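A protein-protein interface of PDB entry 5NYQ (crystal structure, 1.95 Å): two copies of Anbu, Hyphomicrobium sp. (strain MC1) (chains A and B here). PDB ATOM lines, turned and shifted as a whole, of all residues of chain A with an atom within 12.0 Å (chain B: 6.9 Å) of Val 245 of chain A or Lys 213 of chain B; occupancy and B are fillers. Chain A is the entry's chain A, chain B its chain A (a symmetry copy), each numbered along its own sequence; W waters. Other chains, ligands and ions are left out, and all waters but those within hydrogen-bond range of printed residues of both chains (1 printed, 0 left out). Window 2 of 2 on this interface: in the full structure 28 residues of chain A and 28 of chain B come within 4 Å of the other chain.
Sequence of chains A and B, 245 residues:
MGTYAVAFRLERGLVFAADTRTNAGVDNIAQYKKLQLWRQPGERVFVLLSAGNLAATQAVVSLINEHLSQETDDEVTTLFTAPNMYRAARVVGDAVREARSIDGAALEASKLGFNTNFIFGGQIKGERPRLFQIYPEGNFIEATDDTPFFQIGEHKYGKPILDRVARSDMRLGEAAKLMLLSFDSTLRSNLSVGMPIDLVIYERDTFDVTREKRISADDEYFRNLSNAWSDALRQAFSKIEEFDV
No position is printed for both chains.
Of chain B, only Lys 177, Leu 180, Lys 213, Tyr 221 and Phe 222 come within 4 Å of Val 245 of chain A. Of the printed residues of chain A, Lys 213 of chain B touches Val 245 (2.8 Å). No residue of chain A comes within 4 Å of Ala 176 of chain B. Of the printed residues of chain A, Lys 177 of chain B touches Glu 241, Phe 243 and Val 245. No residue of chain A comes within 4 Å of Asp 198 of chain B. No residue of chain A comes within 4 Å of Glu 212 of chain B. Ile 215 of chain B touches none of the printed residues of chain A. Printed residues of chain A within 4 Å of Tyr 221 of chain B: Asp 244 (3.7 Å) and Val 245 (3.9 Å). Phe 222 of chain B touches just one residue of chain A: Val 245. Printed residues of chain A within 4 Å of Leu 225 of chain B: Ile 240. Of the printed residues of chain B, Ile 240 of chain A touches Leu 225. Printed residues of chain B within 4 Å of Phe 243 of chain A: Lys 177 (3.1 Å). Arg 223 of chain B touches none of the printed residues of chain A. The nearest residue of chain A that does not touch Lys 213 of chain B is Asp 244 of chain A (5.8 Å). The nearest printed residue of chain A that does not touch Leu 225 of chain B is Phe 243 of chain A (4.04 Å).
Water W1 bridges the backbone carbonyl oxygen of Asp 244 of chain A (2.9 Å) and the backbone carbonyl oxygen of Tyr 221 of chain B (3.2 Å).
The backbone NH (N) of Tyr 221 of chain B lies close to the side-chain carboxylate (OD2) of Asp 219 of chain B (3.5 Å). OD2 of Asp 219 of chain B is in hydrogen-bond range of N of Phe 222 of chain B (2.9 Å). The backbone NH (N) of Leu 199 of chain B sits at hydrogen-bond distance from the backbone carbonyl oxygen (O) of Lys 213 of chain B, at 2.7 Å.
NZ of Lys 177 of chain B sits at hydrogen-bond distance from O of Glu 241 of chain A (2.7 Å). O of Phe 243 of chain A lies within hydrogen-bond range of NZ of Lys 177 of chain B, 3.1 Å away. NZ of Lys 213 of chain B lies within salt-bridge range of O of Val 245 of chain A, 2.8 Å away.
Among the printed residues, pairs that only touch across the chains: Ile 240 of chain A with Leu 225 of chain B (3.6 Å), Val 245 of chain A with Leu 180 of chain B (3.7 Å), Asp 244 of chain A with Tyr 221 of chain B (3.7 Å), Val 245 of chain A with Lys 177 of chain B (3.8 Å), Val 245 of chain A with Phe 222 of chain B (3.8 Å) and Val 245 of chain A with Tyr 221 of chain B (3.9 Å).
Hydrophobic or aromatic side chains of chain B within 4 Å of the printed part of chain A: Leu 180, Tyr 221, Phe 222 and Leu 225. Of the 9 printed residues of chain A, 5 touch a printed residue of chain B. Hydrophobic or aromatic side chains of chain A within 4 Å of the printed part of chain B: Ile 240 and Val 245. Along chain A the printed residues that touch a printed residue of chain B span positions 240 to 245.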
ATOM      1  N   ARG A 164     -28.070  -3.473 -31.678  1.00  0.00           N
ATOM      2  CA  ARG A 164     -28.026  -4.825 -31.109  1.00  0.00           C
ATOM      3  C   ARG A 164     -29.300  -5.234 -30.353  1.00  0.00           C
ATOM      4  O   ARG A 164     -29.642  -6.420 -30.324  1.00  0.00           O
ATOM      5  CB  ARG A 164     -26.813  -4.952 -30.175  1.00  0.00           C
ATOM      6  CG  ARG A 164     -25.458  -4.858 -30.878  1.00  0.00           C
ATOM      7  CD  ARG A 164     -24.332  -4.667 -29.868  1.00  0.00           C
ATOM      8  NE  ARG A 164     -23.002  -4.509 -30.469  1.00  0.00           N
ATOM      9  CZ  ARG A 164     -22.161  -5.499 -30.794  1.00  0.00           C
ATOM     10  NH1 ARG A 164     -22.473  -6.784 -30.606  1.00  0.00           N
ATOM     11  NH2 ARG A 164     -20.976  -5.198 -31.322  1.00  0.00           N
ATOM     12  N   PHE A 237     -21.016  -7.873 -19.356  1.00  0.00           N
ATOM     13  CA  PHE A 237     -19.602  -7.966 -19.700  1.00  0.00           C
ATOM     14  C   PHE A 237     -18.902  -9.086 -18.924  1.00  0.00           C
ATOM     15  O   PHE A 237     -18.081  -9.809 -19.491  1.00  0.00           O
ATOM     16  CB  PHE A 237     -18.869  -6.639 -19.494  1.00  0.00           C
ATOM     17  CG  PHE A 237     -17.451  -6.680 -19.972  1.00  0.00           C
ATOM     18  CD1 PHE A 237     -17.178  -6.739 -21.334  1.00  0.00           C
ATOM     19  CD2 PHE A 237     -16.395  -6.731 -19.071  1.00  0.00           C
ATOM     20  CE1 PHE A 237     -15.867  -6.812 -21.788  1.00  0.00           C
ATOM     21  CE2 PHE A 237     -15.087  -6.807 -19.518  1.00  0.00           C
ATOM     22  CZ  PHE A 237     -14.826  -6.846 -20.879  1.00  0.00           C
ATOM     23  N   LYS A 239     -20.166 -11.896 -18.029  1.00  0.00           N
ATOM     24  CA  LYS A 239     -20.517 -13.167 -18.678  1.00  0.00           C
ATOM     25  C   LYS A 239     -19.610 -13.422 -19.883  1.00  0.00           C
ATOM     26  O   LYS A 239     -18.920 -14.442 -19.952  1.00  0.00           O
ATOM     27  CB  LYS A 239     -21.978 -13.162 -19.141  1.00  0.00           C
ATOM     28  CG  LYS A 239     -23.015 -13.077 -18.031  1.00  0.00           C
ATOM     29  CD  LYS A 239     -23.351 -14.433 -17.425  1.00  0.00           C
ATOM     30  CE  LYS A 239     -24.634 -14.359 -16.609  1.00  0.00           C
ATOM     31  NZ  LYS A 239     -24.882 -15.610 -15.840  1.00  0.00           N
ATOM     32  N   ILE A 240     -19.601 -12.464 -20.808  1.00  0.00           N
ATOM     33  CA  ILE A 240     -18.976 -12.640 -22.124  1.00  0.00           C
ATOM     34  C   ILE A 240     -17.447 -12.539 -22.155  1.00  0.00           C
ATOM     35  O   ILE A 240     -16.836 -12.857 -23.180  1.00  0.00           O
ATOM     36  CB  ILE A 240     -19.576 -11.674 -23.180  1.00  0.00           C
ATOM     37  CG1 ILE A 240     -19.234 -10.204 -22.875  1.00  0.00           C
ATOM     38  CG2 ILE A 240     -21.081 -11.885 -23.296  1.00  0.00           C
ATOM     39  CD1 ILE A 240     -18.133  -9.624 -23.731  1.00  0.00           C
ATOM     40  N   GLU A 241     -16.824 -12.097 -21.062  1.00  0.00           N
ATOM     41  CA  GLU A 241     -15.363 -12.123 -20.976  1.00  0.00           C
ATOM     42  C   GLU A 241     -14.806 -13.560 -20.880  1.00  0.00           C
ATOM     43  O   GLU A 241     -13.607 -13.754 -21.023  1.00  0.00           O
ATOM     44  CB  GLU A 241     -14.847 -11.216 -19.854  1.00  0.00           C
ATOM     45  CG  GLU A 241     -15.090 -11.707 -18.440  1.00  0.00           C
ATOM     46  CD  GLU A 241     -14.892 -10.620 -17.394  1.00  0.00           C
ATOM     47  OE1 GLU A 241     -14.443  -9.512 -17.740  1.00  0.00           O
ATOM     48  OE2 GLU A 241     -15.187 -10.877 -16.213  1.00  0.00           O
ATOM     49  N   GLU A 242     -15.683 -14.547 -20.655  1.00  0.00           N
ATOM     50  CA  GLU A 242     -15.404 -15.971 -20.953  1.00  0.00           C
ATOM     51  C   GLU A 242     -14.763 -16.219 -22.324  1.00  0.00           C
ATOM     52  O   GLU A 242     -13.960 -17.140 -22.464  1.00  0.00           O
ATOM     53  CB  GLU A 242     -16.699 -16.795 -20.914  1.00  0.00           C
ATOM     54  CG  GLU A 242     -17.179 -17.193 -19.529  1.00  0.00           C
ATOM     55  CD  GLU A 242     -18.489 -17.972 -19.560  1.00  0.00           C
ATOM     56  OE1 GLU A 242     -19.130 -18.059 -20.634  1.00  0.00           O
ATOM     57  OE2 GLU A 242     -18.885 -18.501 -18.498  1.00  0.00           O
ATOM     58  N   PHE A 243     -15.152 -15.433 -23.329  1.00  0.00           N
ATOM     59  CA  PHE A 243     -14.700 -15.635 -24.705  1.00  0.00           C
ATOM     60  C   PHE A 243     -13.374 -14.947 -25.012  1.00  0.00           C
ATOM     61  O   PHE A 243     -13.152 -13.797 -24.629  1.00  0.00           O
ATOM     62  CB  PHE A 243     -15.780 -15.182 -25.686  1.00  0.00           C
ATOM     63  CG  PHE A 243     -17.061 -15.962 -25.561  1.00  0.00           C
ATOM     64  CD1 PHE A 243     -17.113 -17.301 -25.946  1.00  0.00           C
ATOM     65  CD2 PHE A 243     -18.210 -15.374 -25.046  1.00  0.00           C
ATOM     66  CE1 PHE A 243     -18.289 -18.031 -25.830  1.00  0.00           C
ATOM     67  CE2 PHE A 243     -19.385 -16.100 -24.926  1.00  0.00           C
ATOM     68  CZ  PHE A 243     -19.426 -17.429 -25.319  1.00  0.00           C
ATOM     69  N   ASP A 244     -12.508 -15.663 -25.722  1.00  0.00           N
ATOM     70  CA  ASP A 244     -11.175 -15.180 -26.065  1.00  0.00           C
ATOM     71  C   ASP A 244     -11.222 -14.325 -27.328  1.00  0.00           C
ATOM     72  O   ASP A 244     -12.190 -14.376 -28.092  1.00  0.00           O
ATOM     73  CB  ASP A 244     -10.226 -16.373 -26.266  1.00  0.00           C
ATOM     74  CG  ASP A 244      -8.772 -16.036 -25.987  1.00  0.00           C
ATOM     75  OD1 ASP A 244      -8.389 -14.845 -26.018  1.00  0.00           O
ATOM     76  OD2 ASP A 244      -8.004 -16.991 -25.741  1.00  0.00           O
ATOM     77  N   VAL A 245     -10.174 -13.526 -27.523  1.00  0.00           N
ATOM     78  CA  VAL A 245      -9.989 -12.749 -28.751  1.00  0.00           C
ATOM     79  C   VAL A 245      -8.501 -12.447 -28.978  1.00  0.00           C
ATOM     80  O   VAL A 245      -8.072 -12.127 -30.086  1.00  0.00           O
ATOM     81  CB  VAL A 245     -10.831 -11.448 -28.722  1.00  0.00           C
ATOM     82  CG1 VAL A 245     -10.238 -10.421 -27.759  1.00  0.00           C
ATOM     83  CG2 VAL A 245     -10.989 -10.866 -30.119  1.00  0.00           C
ATOM     84  OXT VAL A 245      -7.680 -12.523 -28.060  1.00  0.00           O
ATOM     85  N   GLY B 173      -6.335  -8.342 -20.668  1.00  0.00           N
ATOM     86  CA  GLY B 173      -7.156  -9.012 -21.666  1.00  0.00           C
ATOM     87  C   GLY B 173      -8.622  -8.626 -21.621  1.00  0.00           C
ATOM     88  O   GLY B 173      -9.240  -8.484 -22.665  1.00  0.00           O
ATOM     89  N   ALA B 176      -8.898  -5.141 -23.031  1.00  0.00           N
ATOM     90  CA  ALA B 176      -8.788  -5.279 -24.485  1.00  0.00           C
ATOM     91  C   ALA B 176     -10.121  -5.677 -25.120  1.00  0.00           C
ATOM     92  O   ALA B 176     -10.535  -5.091 -26.127  1.00  0.00           O
ATOM     93  CB  ALA B 176      -7.706  -6.292 -24.840  1.00  0.00           C
ATOM     94  N   LYS B 177     -10.800  -6.652 -24.513  1.00  0.00           N
ATOM     95  CA  LYS B 177     -12.105  -7.104 -24.998  1.00  0.00           C
ATOM     96  C   LYS B 177     -13.133  -5.986 -24.964  1.00  0.00           C
ATOM     97  O   LYS B 177     -13.842  -5.773 -25.945  1.00  0.00           O
ATOM     98  CB  LYS B 177     -12.606  -8.299 -24.191  1.00  0.00           C
ATOM     99  CG  LYS B 177     -11.818  -9.578 -24.431  1.00  0.00           C
ATOM    100  CD  LYS B 177     -12.148 -10.632 -23.387  1.00  0.00           C
ATOM    101  CE  LYS B 177     -11.113 -11.743 -23.373  1.00  0.00           C
ATOM    102  NZ  LYS B 177     -11.432 -12.749 -22.320  1.00  0.00           N
ATOM    103  N   LEU B 180     -12.249  -3.473 -27.728  1.00  0.00           N
ATOM    104  CA  LEU B 180     -12.578  -4.014 -29.054  1.00  0.00           C
ATOM    105  C   LEU B 180     -14.067  -3.936 -29.373  1.00  0.00           C
ATOM    106  O   LEU B 180     -14.436  -3.658 -30.514  1.00  0.00           O
ATOM    107  CB  LEU B 180     -12.079  -5.461 -29.206  1.00  0.00           C
ATOM    108  CG  LEU B 180     -10.570  -5.622 -29.401  1.00  0.00           C
ATOM    109  CD1 LEU B 180     -10.180  -7.090 -29.347  1.00  0.00           C
ATOM    110  CD2 LEU B 180     -10.105  -4.995 -30.710  1.00  0.00           C
ATOM    111  N   ILE B 197      -8.141  -3.667 -36.876  1.00  0.00           N
ATOM    112  CA  ILE B 197      -7.805  -2.974 -35.624  1.00  0.00           C
ATOM    113  C   ILE B 197      -6.421  -3.421 -35.152  1.00  0.00           C
ATOM    114  O   ILE B 197      -6.190  -4.614 -34.988  1.00  0.00           O
ATOM    115  CB  ILE B 197      -8.840  -3.280 -34.510  1.00  0.00           C
ATOM    116  CG1 ILE B 197     -10.261  -2.906 -34.961  1.00  0.00           C
ATOM    117  CG2 ILE B 197      -8.499  -2.523 -33.227  1.00  0.00           C
ATOM    118  CD1 ILE B 197     -11.359  -3.607 -34.189  1.00  0.00           C
ATOM    119  N   ASP B 198      -5.513  -2.463 -34.951  1.00  0.00           N
ATOM    120  CA  ASP B 198      -4.200  -2.726 -34.343  1.00  0.00           C
ATOM    121  C   ASP B 198      -4.344  -2.626 -32.829  1.00  0.00           C
ATOM    122  O   ASP B 198      -4.752  -1.586 -32.324  1.00  0.00           O
ATOM    123  CB  ASP B 198      -3.139  -1.719 -34.824  1.00  0.00           C
ATOM    124  CG  ASP B 198      -2.702  -1.948 -36.271  1.00  0.00           C
ATOM    125  OD1 ASP B 198      -2.002  -1.067 -36.822  1.00  0.00           O
ATOM    126  OD2 ASP B 198      -3.037  -2.997 -36.862  1.00  0.00           O
ATOM    127  N   LEU B 199      -4.001  -3.705 -32.124  1.00  0.00           N
ATOM    128  CA  LEU B 199      -4.147  -3.802 -30.671  1.00  0.00           C
ATOM    129  C   LEU B 199      -2.784  -4.084 -30.057  1.00  0.00           C
ATOM    130  O   LEU B 199      -2.087  -5.005 -30.489  1.00  0.00           O
ATOM    131  CB  LEU B 199      -5.117  -4.930 -30.312  1.00  0.00           C
ATOM    132  CG  LEU B 199      -5.262  -5.342 -28.838  1.00  0.00           C
ATOM    133  CD1 LEU B 199      -5.999  -4.277 -28.041  1.00  0.00           C
ATOM    134  CD2 LEU B 199      -5.987  -6.674 -28.742  1.00  0.00           C
ATOM    135  N   VAL B 200      -2.417  -3.289 -29.059  1.00  0.00           N
ATOM    136  CA  VAL B 200      -1.193  -3.489 -28.291  1.00  0.00           C
ATOM    137  C   VAL B 200      -1.560  -3.591 -26.818  1.00  0.00           C
ATOM    138  O   VAL B 200      -2.227  -2.704 -26.283  1.00  0.00           O
ATOM    139  CB  VAL B 200      -0.213  -2.321 -28.498  1.00  0.00           C
ATOM    140  CG1 VAL B 200       0.880  -2.299 -27.428  1.00  0.00           C
ATOM    141  CG2 VAL B 200       0.407  -2.413 -29.877  1.00  0.00           C
ATOM    142  N   ILE B 201      -1.112  -4.669 -26.174  1.00  0.00           N
ATOM    143  CA  ILE B 201      -1.209  -4.813 -24.728  1.00  0.00           C
ATOM    144  C   ILE B 201       0.189  -4.625 -24.175  1.00  0.00           C
ATOM    145  O   ILE B 201       1.112  -5.329 -24.577  1.00  0.00           O
ATOM    146  CB  ILE B 201      -1.762  -6.199 -24.324  1.00  0.00           C
ATOM    147  CG1 ILE B 201      -3.227  -6.307 -24.760  1.00  0.00           C
ATOM    148  CG2 ILE B 201      -1.619  -6.422 -22.817  1.00  0.00           C
ATOM    149  CD1 ILE B 201      -3.817  -7.702 -24.666  1.00  0.00           C
ATOM    150  N   THR B 210       5.425  -6.965 -26.777  1.00  0.00           N
ATOM    151  CA  THR B 210       5.378  -8.287 -27.400  1.00  0.00           C
ATOM    152  C   THR B 210       3.955  -8.639 -27.858  1.00  0.00           C
ATOM    153  O   THR B 210       3.771  -9.174 -28.955  1.00  0.00           O
ATOM    154  CB  THR B 210       5.905  -9.373 -26.436  1.00  0.00           C
ATOM    155  OG1 THR B 210       5.041  -9.481 -25.295  1.00  0.00           O
ATOM    156  CG2 THR B 210       7.320  -9.042 -25.973  1.00  0.00           C
ATOM    157  N   ARG B 211       2.962  -8.337 -27.018  1.00  0.00           N
ATOM    158  CA  ARG B 211       1.556  -8.621 -27.327  1.00  0.00           C
ATOM    159  C   ARG B 211       0.981  -7.556 -28.262  1.00  0.00           C
ATOM    160  O   ARG B 211       0.302  -6.614 -27.830  1.00  0.00           O
ATOM    161  CB  ARG B 211       0.736  -8.755 -26.039  1.00  0.00           C
ATOM    162  CG  ARG B 211       1.123  -9.982 -25.223  1.00  0.00           C
ATOM    163  CD  ARG B 211       0.552  -9.972 -23.815  1.00  0.00           C
ATOM    164  NE  ARG B 211      -0.887 -10.240 -23.785  1.00  0.00           N
ATOM    165  CZ  ARG B 211      -1.624 -10.340 -22.677  1.00  0.00           C
ATOM    166  NH1 ARG B 211      -1.074 -10.202 -21.470  1.00  0.00           N
ATOM    167  NH2 ARG B 211      -2.928 -10.579 -22.773  1.00  0.00           N
ATOM    168  N   GLU B 212       1.284  -7.728 -29.549  1.00  0.00           N
ATOM    169  CA  GLU B 212       0.838  -6.849 -30.632  1.00  0.00           C
ATOM    170  C   GLU B 212      -0.031  -7.701 -31.551  1.00  0.00           C
ATOM    171  O   GLU B 212       0.347  -8.827 -31.878  1.00  0.00           O
ATOM    172  CB  GLU B 212       2.059  -6.310 -31.390  1.00  0.00           C
ATOM    173  CG  GLU B 212       1.831  -5.026 -32.183  1.00  0.00           C
ATOM    174  CD  GLU B 212       1.096  -5.222 -33.497  1.00  0.00           C
ATOM    175  OE1 GLU B 212       1.379  -6.204 -34.218  1.00  0.00           O
ATOM    176  OE2 GLU B 212       0.239  -4.370 -33.819  1.00  0.00           O
ATOM    177  N   LYS B 213      -1.181  -7.176 -31.972  1.00  0.00           N
ATOM    178  CA  LYS B 213      -2.158  -7.975 -32.718  1.00  0.00           C
ATOM    179  C   LYS B 213      -2.993  -7.149 -33.697  1.00  0.00           C
ATOM    180  O   LYS B 213      -3.507  -6.092 -33.340  1.00  0.00           O
ATOM    181  CB  LYS B 213      -3.085  -8.687 -31.733  1.00  0.00           C
ATOM    182  CG  LYS B 213      -3.822  -9.875 -32.318  1.00  0.00           C
ATOM    183  CD  LYS B 213      -4.517 -10.666 -31.225  1.00  0.00           C
ATOM    184  CE  LYS B 213      -5.033 -11.997 -31.740  1.00  0.00           C
ATOM    185  NZ  LYS B 213      -5.471 -12.857 -30.610  1.00  0.00           N
ATOM    186  N   ARG B 214      -3.121  -7.646 -34.927  1.00  0.00           N
ATOM    187  CA  ARG B 214      -4.022  -7.064 -35.919  1.00  0.00           C
ATOM    188  C   ARG B 214      -5.270  -7.939 -36.008  1.00  0.00           C
ATOM    189  O   ARG B 214      -5.169  -9.134 -36.278  1.00  0.00           O
ATOM    190  CB  ARG B 214      -3.333  -6.962 -37.281  1.00  0.00           C
ATOM    191  CG  ARG B 214      -4.149  -6.213 -38.327  1.00  0.00           C
ATOM    192  CD  ARG B 214      -3.276  -5.698 -39.461  1.00  0.00           C
ATOM    193  NE  ARG B 214      -2.443  -4.568 -39.048  1.00  0.00           N
ATOM    194  CZ  ARG B 214      -1.561  -3.940 -39.826  1.00  0.00           C
ATOM    195  NH1 ARG B 214      -1.366  -4.314 -41.092  1.00  0.00           N
ATOM    196  NH2 ARG B 214      -0.857  -2.921 -39.335  1.00  0.00           N
ATOM    197  N   ILE B 215      -6.436  -7.340 -35.773  1.00  0.00           N
ATOM    198  CA  ILE B 215      -7.711  -8.062 -35.759  1.00  0.00           C
ATOM    199  C   ILE B 215      -8.570  -7.552 -36.912  1.00  0.00           C
ATOM    200  O   ILE B 215      -8.931  -6.372 -36.946  1.00  0.00           O
ATOM    201  CB  ILE B 215      -8.448  -7.870 -34.414  1.00  0.00           C
ATOM    202  CG1 ILE B 215      -7.580  -8.382 -33.256  1.00  0.00           C
ATOM    203  CG2 ILE B 215      -9.783  -8.613 -34.411  1.00  0.00           C
ATOM    204  CD1 ILE B 215      -7.944  -7.804 -31.908  1.00  0.00           C
ATOM    205  N   ASP B 219     -12.056 -12.101 -38.379  1.00  0.00           N
ATOM    206  CA  ASP B 219     -11.554 -12.836 -37.217  1.00  0.00           C
ATOM    207  C   ASP B 219     -12.713 -13.512 -36.485  1.00  0.00           C
ATOM    208  O   ASP B 219     -13.606 -12.836 -35.971  1.00  0.00           O
ATOM    209  CB  ASP B 219     -10.798 -11.910 -36.263  1.00  0.00           C
ATOM    210  CG  ASP B 219     -10.127 -12.667 -35.138  1.00  0.00           C
ATOM    211  OD1 ASP B 219      -9.118 -13.356 -35.395  1.00  0.00           O
ATOM    212  OD2 ASP B 219     -10.612 -12.579 -33.995  1.00  0.00           O
ATOM    213  N   TYR B 221     -12.789 -15.287 -33.679  1.00  0.00           N
ATOM    214  CA  TYR B 221     -12.808 -15.018 -32.239  1.00  0.00           C
ATOM    215  C   TYR B 221     -13.564 -13.712 -31.961  1.00  0.00           C
ATOM    216  O   TYR B 221     -14.418 -13.660 -31.072  1.00  0.00           O
ATOM    217  CB  TYR B 221     -11.390 -14.916 -31.664  1.00  0.00           C
ATOM    218  CG  TYR B 221     -10.638 -16.225 -31.544  1.00  0.00           C
ATOM    219  CD1 TYR B 221      -9.905 -16.742 -32.616  1.00  0.00           C
ATOM    220  CD2 TYR B 221     -10.627 -16.933 -30.341  1.00  0.00           C
ATOM    221  CE1 TYR B 221      -9.203 -17.935 -32.497  1.00  0.00           C
ATOM    222  CE2 TYR B 221      -9.928 -18.125 -30.214  1.00  0.00           C
ATOM    223  CZ  TYR B 221      -9.219 -18.624 -31.292  1.00  0.00           C
ATOM    224  OH  TYR B 221      -8.526 -19.805 -31.161  1.00  0.00           O
ATOM    225  N   PHE B 222     -13.243 -12.676 -32.733  1.00  0.00           N
ATOM    226  CA  PHE B 222     -13.856 -11.356 -32.572  1.00  0.00           C
ATOM    227  C   PHE B 222     -15.357 -11.374 -32.900  1.00  0.00           C
ATOM    228  O   PHE B 222     -16.153 -10.737 -32.202  1.00  0.00           O
ATOM    229  CB  PHE B 222     -13.105 -10.314 -33.418  1.00  0.00           C
ATOM    230  CG  PHE B 222     -13.645  -8.913 -33.297  1.00  0.00           C
ATOM    231  CD1 PHE B 222     -13.828  -8.322 -32.051  1.00  0.00           C
ATOM    232  CD2 PHE B 222     -13.957  -8.174 -34.436  1.00  0.00           C
ATOM    233  CE1 PHE B 222     -14.324  -7.030 -31.942  1.00  0.00           C
ATOM    234  CE2 PHE B 222     -14.449  -6.879 -34.331  1.00  0.00           C
ATOM    235  CZ  PHE B 222     -14.634  -6.308 -33.083  1.00  0.00           C
ATOM    236  N   ARG B 223     -15.739 -12.122 -33.937  1.00  0.00           N
ATOM    237  CA  ARG B 223     -17.155 -12.319 -34.267  1.00  0.00           C
ATOM    238  C   ARG B 223     -17.910 -13.044 -33.148  1.00  0.00           C
ATOM    239  O   ARG B 223     -19.015 -12.640 -32.782  1.00  0.00           O
ATOM    240  CB  ARG B 223     -17.316 -13.084 -35.588  1.00  0.00           C
ATOM    241  CG  ARG B 223     -16.829 -12.321 -36.819  1.00  0.00           C
ATOM    242  CD  ARG B 223     -17.781 -11.203 -37.229  1.00  0.00           C
ATOM    243  NE  ARG B 223     -19.066 -11.707 -37.722  1.00  0.00           N
ATOM    244  CZ  ARG B 223     -20.102 -10.946 -38.085  1.00  0.00           C
ATOM    245  NH1 ARG B 223     -20.036  -9.614 -38.019  1.00  0.00           N
ATOM    246  NH2 ARG B 223     -21.220 -11.522 -38.518  1.00  0.00           N
ATOM    247  N   LEU B 225     -17.096 -13.128 -29.932  1.00  0.00           N
ATOM    248  CA  LEU B 225     -17.193 -12.167 -28.827  1.00  0.00           C
ATOM    249  C   LEU B 225     -18.331 -11.169 -29.059  1.00  0.00           C
ATOM    250  O   LEU B 225     -19.131 -10.918 -28.152  1.00  0.00           O
ATOM    251  CB  LEU B 225     -15.871 -11.415 -28.648  1.00  0.00           C
ATOM    252  CG  LEU B 225     -15.746 -10.426 -27.486  1.00  0.00           C
ATOM    253  CD1 LEU B 225     -15.802 -11.148 -26.151  1.00  0.00           C
ATOM    254  CD2 LEU B 225     -14.456  -9.628 -27.616  1.00  0.00           C
HETATM  255  O   HOH W   1     -14.256 -16.114 -29.020  1.00  0.00           O
